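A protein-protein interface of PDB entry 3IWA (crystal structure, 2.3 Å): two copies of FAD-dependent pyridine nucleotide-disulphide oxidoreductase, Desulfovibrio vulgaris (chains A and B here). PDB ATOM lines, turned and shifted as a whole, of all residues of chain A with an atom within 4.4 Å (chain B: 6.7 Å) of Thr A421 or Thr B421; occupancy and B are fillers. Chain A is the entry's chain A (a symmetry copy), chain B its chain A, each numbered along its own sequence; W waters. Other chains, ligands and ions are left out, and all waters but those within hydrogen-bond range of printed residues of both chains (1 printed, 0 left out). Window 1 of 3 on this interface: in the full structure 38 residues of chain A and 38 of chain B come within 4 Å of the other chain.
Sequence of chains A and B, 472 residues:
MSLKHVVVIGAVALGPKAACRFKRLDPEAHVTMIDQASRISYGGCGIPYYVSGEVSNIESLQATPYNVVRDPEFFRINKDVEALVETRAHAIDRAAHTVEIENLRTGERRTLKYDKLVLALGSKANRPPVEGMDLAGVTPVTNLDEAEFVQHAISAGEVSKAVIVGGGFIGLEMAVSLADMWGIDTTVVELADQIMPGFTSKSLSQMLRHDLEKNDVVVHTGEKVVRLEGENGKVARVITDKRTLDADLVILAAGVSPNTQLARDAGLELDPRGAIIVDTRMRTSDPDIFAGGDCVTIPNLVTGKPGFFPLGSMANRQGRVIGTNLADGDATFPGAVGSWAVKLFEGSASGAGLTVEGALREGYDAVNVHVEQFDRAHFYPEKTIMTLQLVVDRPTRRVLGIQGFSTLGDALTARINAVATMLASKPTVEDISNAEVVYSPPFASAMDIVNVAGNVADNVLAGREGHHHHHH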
ATOM      1  N   ASN A 417      16.388 -32.752  -0.304  1.00  0.00           N
ATOM      2  CA  ASN A 417      17.464 -32.176   0.515  1.00  0.00           C
ATOM      3  C   ASN A 417      17.305 -30.699   0.702  1.00  0.00           C
ATOM      4  O   ASN A 417      17.508 -30.197   1.792  1.00  0.00           O
ATOM      5  CB  ASN A 417      18.828 -32.377  -0.142  1.00  0.00           C
ATOM      6  CG  ASN A 417      19.482 -33.696   0.222  1.00  0.00           C
ATOM      7  OD1 ASN A 417      18.971 -34.462   1.048  1.00  0.00           O
ATOM      8  ND2 ASN A 417      20.648 -33.952  -0.382  1.00  0.00           N
ATOM      9  N   ALA A 418      16.962 -30.005  -0.387  1.00  0.00           N
ATOM     10  CA  ALA A 418      16.811 -28.552  -0.351  1.00  0.00           C
ATOM     11  C   ALA A 418      15.873 -28.157   0.746  1.00  0.00           C
ATOM     12  O   ALA A 418      16.129 -27.184   1.457  1.00  0.00           O
ATOM     13  CB  ALA A 418      16.314 -27.994  -1.696  1.00  0.00           C
ATOM     14  N   VAL A 419      14.759 -28.865   0.846  1.00  0.00           N
ATOM     15  CA  VAL A 419      13.755 -28.541   1.829  1.00  0.00           C
ATOM     16  C   VAL A 419      14.057 -29.154   3.216  1.00  0.00           C
ATOM     17  O   VAL A 419      13.802 -28.519   4.244  1.00  0.00           O
ATOM     18  CB  VAL A 419      12.356 -28.969   1.308  1.00  0.00           C
ATOM     19  CG1 VAL A 419      11.323 -28.729   2.352  1.00  0.00           C
ATOM     20  CG2 VAL A 419      12.022 -28.256  -0.043  1.00  0.00           C
ATOM     21  N   ALA A 420      14.618 -30.354   3.249  1.00  0.00           N
ATOM     22  CA  ALA A 420      14.896 -31.067   4.522  1.00  0.00           C
ATOM     23  C   ALA A 420      15.794 -30.270   5.471  1.00  0.00           C
ATOM     24  O   ALA A 420      15.545 -30.198   6.698  1.00  0.00           O
ATOM     25  CB  ALA A 420      15.509 -32.477   4.245  1.00  0.00           C
ATOM     26  N   THR A 421      16.844 -29.661   4.914  1.00  0.00           N
ATOM     27  CA  THR A 421      17.731 -28.841   5.721  1.00  0.00           C
ATOM     28  C   THR A 421      17.102 -27.509   6.133  1.00  0.00           C
ATOM     29  O   THR A 421      17.610 -26.830   7.034  1.00  0.00           O
ATOM     30  CB  THR A 421      19.054 -28.572   5.013  1.00  0.00           C
ATOM     31  OG1 THR A 421      18.828 -27.840   3.782  1.00  0.00           O
ATOM     32  CG2 THR A 421      19.762 -29.907   4.732  1.00  0.00           C
ATOM     33  N   MET A 422      15.984 -27.151   5.501  1.00  0.00           N
ATOM     34  CA  MET A 422      15.249 -25.960   5.874  1.00  0.00           C
ATOM     35  C   MET A 422      14.260 -26.257   7.011  1.00  0.00           C
ATOM     36  O   MET A 422      13.901 -25.332   7.736  1.00  0.00           O
ATOM     37  CB  MET A 422      14.451 -25.373   4.670  1.00  0.00           C
ATOM     38  CG  MET A 422      15.197 -25.135   3.307  1.00  0.00           C
ATOM     39  SD  MET A 422      14.175 -24.538   1.883  1.00  0.00           S
ATOM     40  CE  MET A 422      13.524 -23.177   2.793  1.00  0.00           C
ATOM     41  N   LEU A 423      13.762 -27.503   7.141  1.00  0.00           N
ATOM     42  CA  LEU A 423      12.590 -27.755   8.038  1.00  0.00           C
ATOM     43  C   LEU A 423      12.793 -27.293   9.470  1.00  0.00           C
ATOM     44  O   LEU A 423      11.901 -26.693  10.042  1.00  0.00           O
ATOM     45  CB  LEU A 423      12.140 -29.214   8.046  1.00  0.00           C
ATOM     46  CG  LEU A 423      11.557 -29.702   6.716  1.00  0.00           C
ATOM     47  CD1 LEU A 423      11.234 -31.212   6.776  1.00  0.00           C
ATOM     48  CD2 LEU A 423      10.341 -28.899   6.322  1.00  0.00           C
ATOM     49  N   GLU A 436      16.195 -20.981  -2.757  1.00  0.00           N
ATOM     50  CA  GLU A 436      17.189 -20.598  -3.753  1.00  0.00           C
ATOM     51  C   GLU A 436      17.922 -21.837  -4.243  1.00  0.00           C
ATOM     52  O   GLU A 436      19.120 -22.025  -4.025  1.00  0.00           O
ATOM     53  CB  GLU A 436      18.129 -19.483  -3.264  1.00  0.00           C
ATOM     54  CG  GLU A 436      18.821 -18.869  -4.442  1.00  0.00           C
ATOM     55  CD  GLU A 436      19.768 -17.729  -4.120  1.00  0.00           C
ATOM     56  OE1 GLU A 436      19.755 -17.208  -2.986  1.00  0.00           O
ATOM     57  OE2 GLU A 436      20.514 -17.332  -5.048  1.00  0.00           O
ATOM     58  N   VAL A 437      17.150 -22.680  -4.909  1.00  0.00           N
ATOM     59  CA  VAL A 437      17.651 -23.920  -5.425  1.00  0.00           C
ATOM     60  C   VAL A 437      18.344 -23.648  -6.724  1.00  0.00           C
ATOM     61  O   VAL A 437      17.992 -22.744  -7.470  1.00  0.00           O
ATOM     62  CB  VAL A 437      16.567 -25.002  -5.608  1.00  0.00           C
ATOM     63  CG1 VAL A 437      15.877 -25.295  -4.258  1.00  0.00           C
ATOM     64  CG2 VAL A 437      15.551 -24.607  -6.675  1.00  0.00           C
ATOM     65  N   VAL B 337      21.657 -15.526  -2.118  1.00  0.00           N
ATOM     66  CA  VAL B 337      22.996 -16.010  -1.872  1.00  0.00           C
ATOM     67  C   VAL B 337      23.768 -16.388  -3.140  1.00  0.00           C
ATOM     68  O   VAL B 337      24.960 -16.650  -3.048  1.00  0.00           O
ATOM     69  CB  VAL B 337      23.004 -17.205  -0.874  1.00  0.00           C
ATOM     70  CG1 VAL B 337      22.337 -16.785   0.449  1.00  0.00           C
ATOM     71  CG2 VAL B 337      22.352 -18.434  -1.472  1.00  0.00           C
ATOM     72  N   SER B 339      23.097 -18.951  -5.789  1.00  0.00           N
ATOM     73  CA  SER B 339      23.139 -20.303  -6.277  1.00  0.00           C
ATOM     74  C   SER B 339      23.253 -20.367  -7.795  1.00  0.00           C
ATOM     75  O   SER B 339      22.639 -19.584  -8.489  1.00  0.00           O
ATOM     76  CB  SER B 339      21.856 -20.993  -5.842  1.00  0.00           C
ATOM     77  OG  SER B 339      21.687 -20.849  -4.454  1.00  0.00           O
ATOM     78  N   ALA B 352      27.080 -21.801  -4.489  1.00  0.00           N
ATOM     79  CA  ALA B 352      26.256 -20.792  -3.844  1.00  0.00           C
ATOM     80  C   ALA B 352      27.132 -20.046  -2.894  1.00  0.00           C
ATOM     81  O   ALA B 352      28.034 -20.625  -2.351  1.00  0.00           O
ATOM     82  CB  ALA B 352      25.066 -21.404  -3.088  1.00  0.00           C
ATOM     83  N   ILE B 416      24.802 -29.433  -3.365  1.00  0.00           N
ATOM     84  CA  ILE B 416      24.798 -27.962  -3.319  1.00  0.00           C
ATOM     85  C   ILE B 416      23.471 -27.367  -2.790  1.00  0.00           C
ATOM     86  O   ILE B 416      23.468 -26.392  -2.025  1.00  0.00           O
ATOM     87  CB  ILE B 416      25.121 -27.359  -4.730  1.00  0.00           C
ATOM     88  CG1 ILE B 416      26.532 -27.758  -5.202  1.00  0.00           C
ATOM     89  CG2 ILE B 416      24.972 -25.854  -4.714  1.00  0.00           C
ATOM     90  CD1 ILE B 416      27.687 -27.480  -4.203  1.00  0.00           C
ATOM     91  N   ASN B 417      22.340 -27.940  -3.213  1.00  0.00           N
ATOM     92  CA  ASN B 417      21.027 -27.455  -2.761  1.00  0.00           C
ATOM     93  C   ASN B 417      20.876 -27.536  -1.274  1.00  0.00           C
ATOM     94  O   ASN B 417      20.358 -26.620  -0.662  1.00  0.00           O
ATOM     95  CB  ASN B 417      19.895 -28.293  -3.349  1.00  0.00           C
ATOM     96  CG  ASN B 417      19.424 -27.800  -4.705  1.00  0.00           C
ATOM     97  OD1 ASN B 417      19.874 -26.762  -5.205  1.00  0.00           O
ATOM     98  ND2 ASN B 417      18.480 -28.541  -5.296  1.00  0.00           N
ATOM     99  N   ALA B 418      21.315 -28.661  -0.701  1.00  0.00           N
ATOM    100  CA  ALA B 418      21.193 -28.884   0.738  1.00  0.00           C
ATOM    101  C   ALA B 418      21.787 -27.736   1.492  1.00  0.00           C
ATOM    102  O   ALA B 418      21.216 -27.286   2.485  1.00  0.00           O
ATOM    103  CB  ALA B 418      21.858 -30.201   1.171  1.00  0.00           C
ATOM    104  N   VAL B 419      22.963 -27.301   1.063  1.00  0.00           N
ATOM    105  CA  VAL B 419      23.658 -26.238   1.744  1.00  0.00           C
ATOM    106  C   VAL B 419      23.180 -24.835   1.305  1.00  0.00           C
ATOM    107  O   VAL B 419      23.092 -23.922   2.133  1.00  0.00           O
ATOM    108  CB  VAL B 419      25.190 -26.407   1.549  1.00  0.00           C
ATOM    109  CG1 VAL B 419      25.915 -25.262   2.166  1.00  0.00           C
ATOM    110  CG2 VAL B 419      25.673 -27.790   2.098  1.00  0.00           C
ATOM    111  N   ALA B 420      22.849 -24.668   0.032  1.00  0.00           N
ATOM    112  CA  ALA B 420      22.437 -23.350  -0.514  1.00  0.00           C
ATOM    113  C   ALA B 420      21.229 -22.752   0.210  1.00  0.00           C
ATOM    114  O   ALA B 420      21.192 -21.538   0.524  1.00  0.00           O
ATOM    115  CB  ALA B 420      22.160 -23.450  -2.049  1.00  0.00           C
ATOM    116  N   THR B 421      20.231 -23.595   0.485  1.00  0.00           N
ATOM    117  CA  THR B 421      19.060 -23.137   1.211  1.00  0.00           C
ATOM    118  C   THR B 421      19.337 -22.888   2.695  1.00  0.00           C
ATOM    119  O   THR B 421      18.534 -22.243   3.381  1.00  0.00           O
ATOM    120  CB  THR B 421      17.893 -24.109   1.077  1.00  0.00           C
ATOM    121  OG1 THR B 421      18.243 -25.400   1.639  1.00  0.00           O
ATOM    122  CG2 THR B 421      17.512 -24.245  -0.406  1.00  0.00           C
ATOM    123  N   MET B 422      20.482 -23.368   3.180  1.00  0.00           N
ATOM    124  CA  MET B 422      20.895 -23.111   4.545  1.00  0.00           C
ATOM    125  C   MET B 422      21.654 -21.780   4.649  1.00  0.00           C
ATOM    126  O   MET B 422      21.678 -21.198   5.731  1.00  0.00           O
ATOM    127  CB  MET B 422      21.815 -24.245   5.094  1.00  0.00           C
ATOM    128  CG  MET B 422      21.347 -25.738   4.950  1.00  0.00           C
ATOM    129  SD  MET B 422      22.528 -27.046   5.522  1.00  0.00           S
ATOM    130  CE  MET B 422      22.715 -26.319   7.116  1.00  0.00           C
ATOM    131  N   LEU B 423      22.328 -21.320   3.574  1.00  0.00           N
ATOM    132  CA  LEU B 423      23.306 -20.197   3.723  1.00  0.00           C
ATOM    133  C   LEU B 423      22.721 -18.944   4.348  1.00  0.00           C
ATOM    134  O   LEU B 423      23.348 -18.351   5.207  1.00  0.00           O
ATOM    135  CB  LEU B 423      23.997 -19.823   2.414  1.00  0.00           C
ATOM    136  CG  LEU B 423      24.929 -20.906   1.860  1.00  0.00           C
ATOM    137  CD1 LEU B 423      25.496 -20.493   0.483  1.00  0.00           C
ATOM    138  CD2 LEU B 423      26.037 -21.226   2.833  1.00  0.00           C
ATOM    139  N   ALA B 424      21.509 -18.571   3.952  1.00  0.00           N
ATOM    140  CA  ALA B 424      20.848 -17.372   4.495  1.00  0.00           C
ATOM    141  C   ALA B 424      20.610 -17.443   5.998  1.00  0.00           C
ATOM    142  O   ALA B 424      20.544 -16.424   6.633  1.00  0.00           O
ATOM    143  CB  ALA B 424      19.503 -17.104   3.768  1.00  0.00           C
ATOM    144  N   SER B 425      20.491 -18.641   6.564  1.00  0.00           N
ATOM    145  CA  SER B 425      20.321 -18.792   8.025  1.00  0.00           C
ATOM    146  C   SER B 425      21.643 -18.756   8.808  1.00  0.00           C
ATOM    147  O   SER B 425      21.645 -18.941  10.016  1.00  0.00           O
ATOM    148  CB  SER B 425      19.571 -20.087   8.334  1.00  0.00           C
ATOM    149  OG  SER B 425      18.229 -19.974   7.869  1.00  0.00           O
ATOM    150  N   ALA B 435      24.080 -31.656   9.008  1.00  0.00           N
ATOM    151  CA  ALA B 435      23.035 -31.388   8.008  1.00  0.00           C
ATOM    152  C   ALA B 435      22.270 -32.653   7.757  1.00  0.00           C
ATOM    153  O   ALA B 435      22.864 -33.679   7.484  1.00  0.00           O
ATOM    154  CB  ALA B 435      23.627 -30.886   6.688  1.00  0.00           C
ATOM    155  N   GLU B 436      20.947 -32.578   7.793  1.00  0.00           N
ATOM    156  CA  GLU B 436      20.138 -33.792   7.794  1.00  0.00           C
ATOM    157  C   GLU B 436      19.760 -34.152   6.365  1.00  0.00           C
ATOM    158  O   GLU B 436      18.597 -34.118   5.961  1.00  0.00           O
ATOM    159  CB  GLU B 436      18.931 -33.706   8.744  1.00  0.00           C
ATOM    160  CG  GLU B 436      18.409 -35.086   9.004  1.00  0.00           C
ATOM    161  CD  GLU B 436      17.227 -35.168   9.950  1.00  0.00           C
ATOM    162  OE1 GLU B 436      16.903 -34.175  10.632  1.00  0.00           O
ATOM    163  OE2 GLU B 436      16.639 -36.274  10.027  1.00  0.00           O
ATOM    164  N   VAL B 437      20.795 -34.490   5.614  1.00  0.00           N
ATOM    165  CA  VAL B 437      20.646 -34.835   4.230  1.00  0.00           C
ATOM    166  C   VAL B 437      20.210 -36.264   4.141  1.00  0.00           C
ATOM    167  O   VAL B 437      20.546 -37.097   4.972  1.00  0.00           O
ATOM    168  CB  VAL B 437      21.920 -34.605   3.391  1.00  0.00           C
ATOM    169  CG1 VAL B 437      22.345 -33.123   3.468  1.00  0.00           C
ATOM    170  CG2 VAL B 437      23.053 -35.529   3.823  1.00  0.00           C
HETATM  171  O   HOH W   1      20.654 -17.872  -7.426  1.00  0.00           O
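Thr A421 touches just these residues of chain B: Ala B418 (2.8 Å), Thr B421 (3.3 Å) and Met B422 (3.5 Å).
Of the printed residues of chain A, Val B337 touches Glu A436 (2.7 Å).
Of the printed residues of chain A, Asn B417 touches Ala A418 and Val A437.
Printed residues of chain A within 4 Å of Ala B418: Asn A417 and Thr A421.
Thr B421 touches just these residues of chain A: Ala A418 (2.8 Å), Thr A421 (3.3 Å) and Met A422 (3.5 Å).
Ala B424 touches none of the printed residues of chain A.
Ser B425 touches none of the printed residues of chain A.
The nearest residue of chain A that does not touch Thr B421 is Glu A436 (4.2 Å).
N of Val B337 sits at hydrogen-bond distance from OE1 of Glu A436, 2.7 Å away.
The side-chain hydroxyl of Ser B339 lies within hydrogen-bond range of the backbone carbonyl oxygen of Glu A436, 2.9 Å away.
The backbone carbonyl oxygen (O) of Ala B418 sits at hydrogen-bond distance from the side-chain hydroxyl (OG1) of Thr A421.
O of Ala A418 lies within hydrogen-bond range of OG1 of Thr B421 (2.8 Å).
The side-chain hydroxyl of Thr A421 lies within hydrogen-bond range of the side-chain hydroxyl of Thr B421 (3.3 Å).
Water W1 bridges OE2 of Glu A436 (2.4 Å) and O of Ser B339 (2.8 Å).
Printed residues of chain A that touch a printed residue of chain B: Asn A417, Ala A418, Ala A420, Thr A421, Met A422, Glu A436 and Val A437.
Hydrophobic or aromatic side chains of chain A that line the printed part of chain B: Ala A418, Ala A420, Met A422 and Val A437.
Of the 16 printed residues of chain B, 9 touch a printed residue of chain A.
Printed residues of chain B that touch a printed residue of chain A: Val B337, Ser B339, Asn B417, Ala B418, Ala B420, Thr B421, Met B422, Glu B436 and Val B437.
Hydrophobic or aromatic side chains of chain B that line the printed part of chain A: Val B337, Ala B418, Ala B420, Met B422 and Val B437.
Among the printed residues, 13 pairs touch across the chains.
Among the printed residues, no Asp or Glu carboxylate lies within 4 Å of a Lys or Arg side-chain nitrogen of the other chain.
Ala B418 touches Asn A417 (CB to CB, 3.95 Å).
Val B437 touches Asn A417 (CA to OD1, 3.6 Å).
Ala A418 touches Asn B417 (CB to CB, 3.96 Å).
Ala A420 touches Glu B436 (CB to O, 3.9 Å).
Thr A421 touches Met B422 (OG1 to CG, 3.5 Å).
Met A422 touches Thr B421 (CG to OG1, 3.5 Å).
Glu A436 touches Ala B420 (O to CB, 3.9 Å).
Asn B417 touches Val A437 (OD1 to CA, 3.6 Å).
The backbone carbonyl oxygen (O) of Asn B417 lies within hydrogen-bond range of the side-chain hydroxyl (OG1) of Thr B421, at 3.4 Å.
The backbone carbonyl oxygen of Asn A417 is in hydrogen-bond range of the side-chain hydroxyl of Thr A421 (3.4 Å).
Asn A417 touches Ala B418, and with the chains exchanged Ala A418 touches Asn B417.
Ala A418 touches Thr B421, and with the chains exchanged Thr A421 touches Ala B418.
Thr A421 touches its own counterpart, Thr B421.
Thr A421 touches Met B422, and with the chains exchanged Met A422 touches Thr B421.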
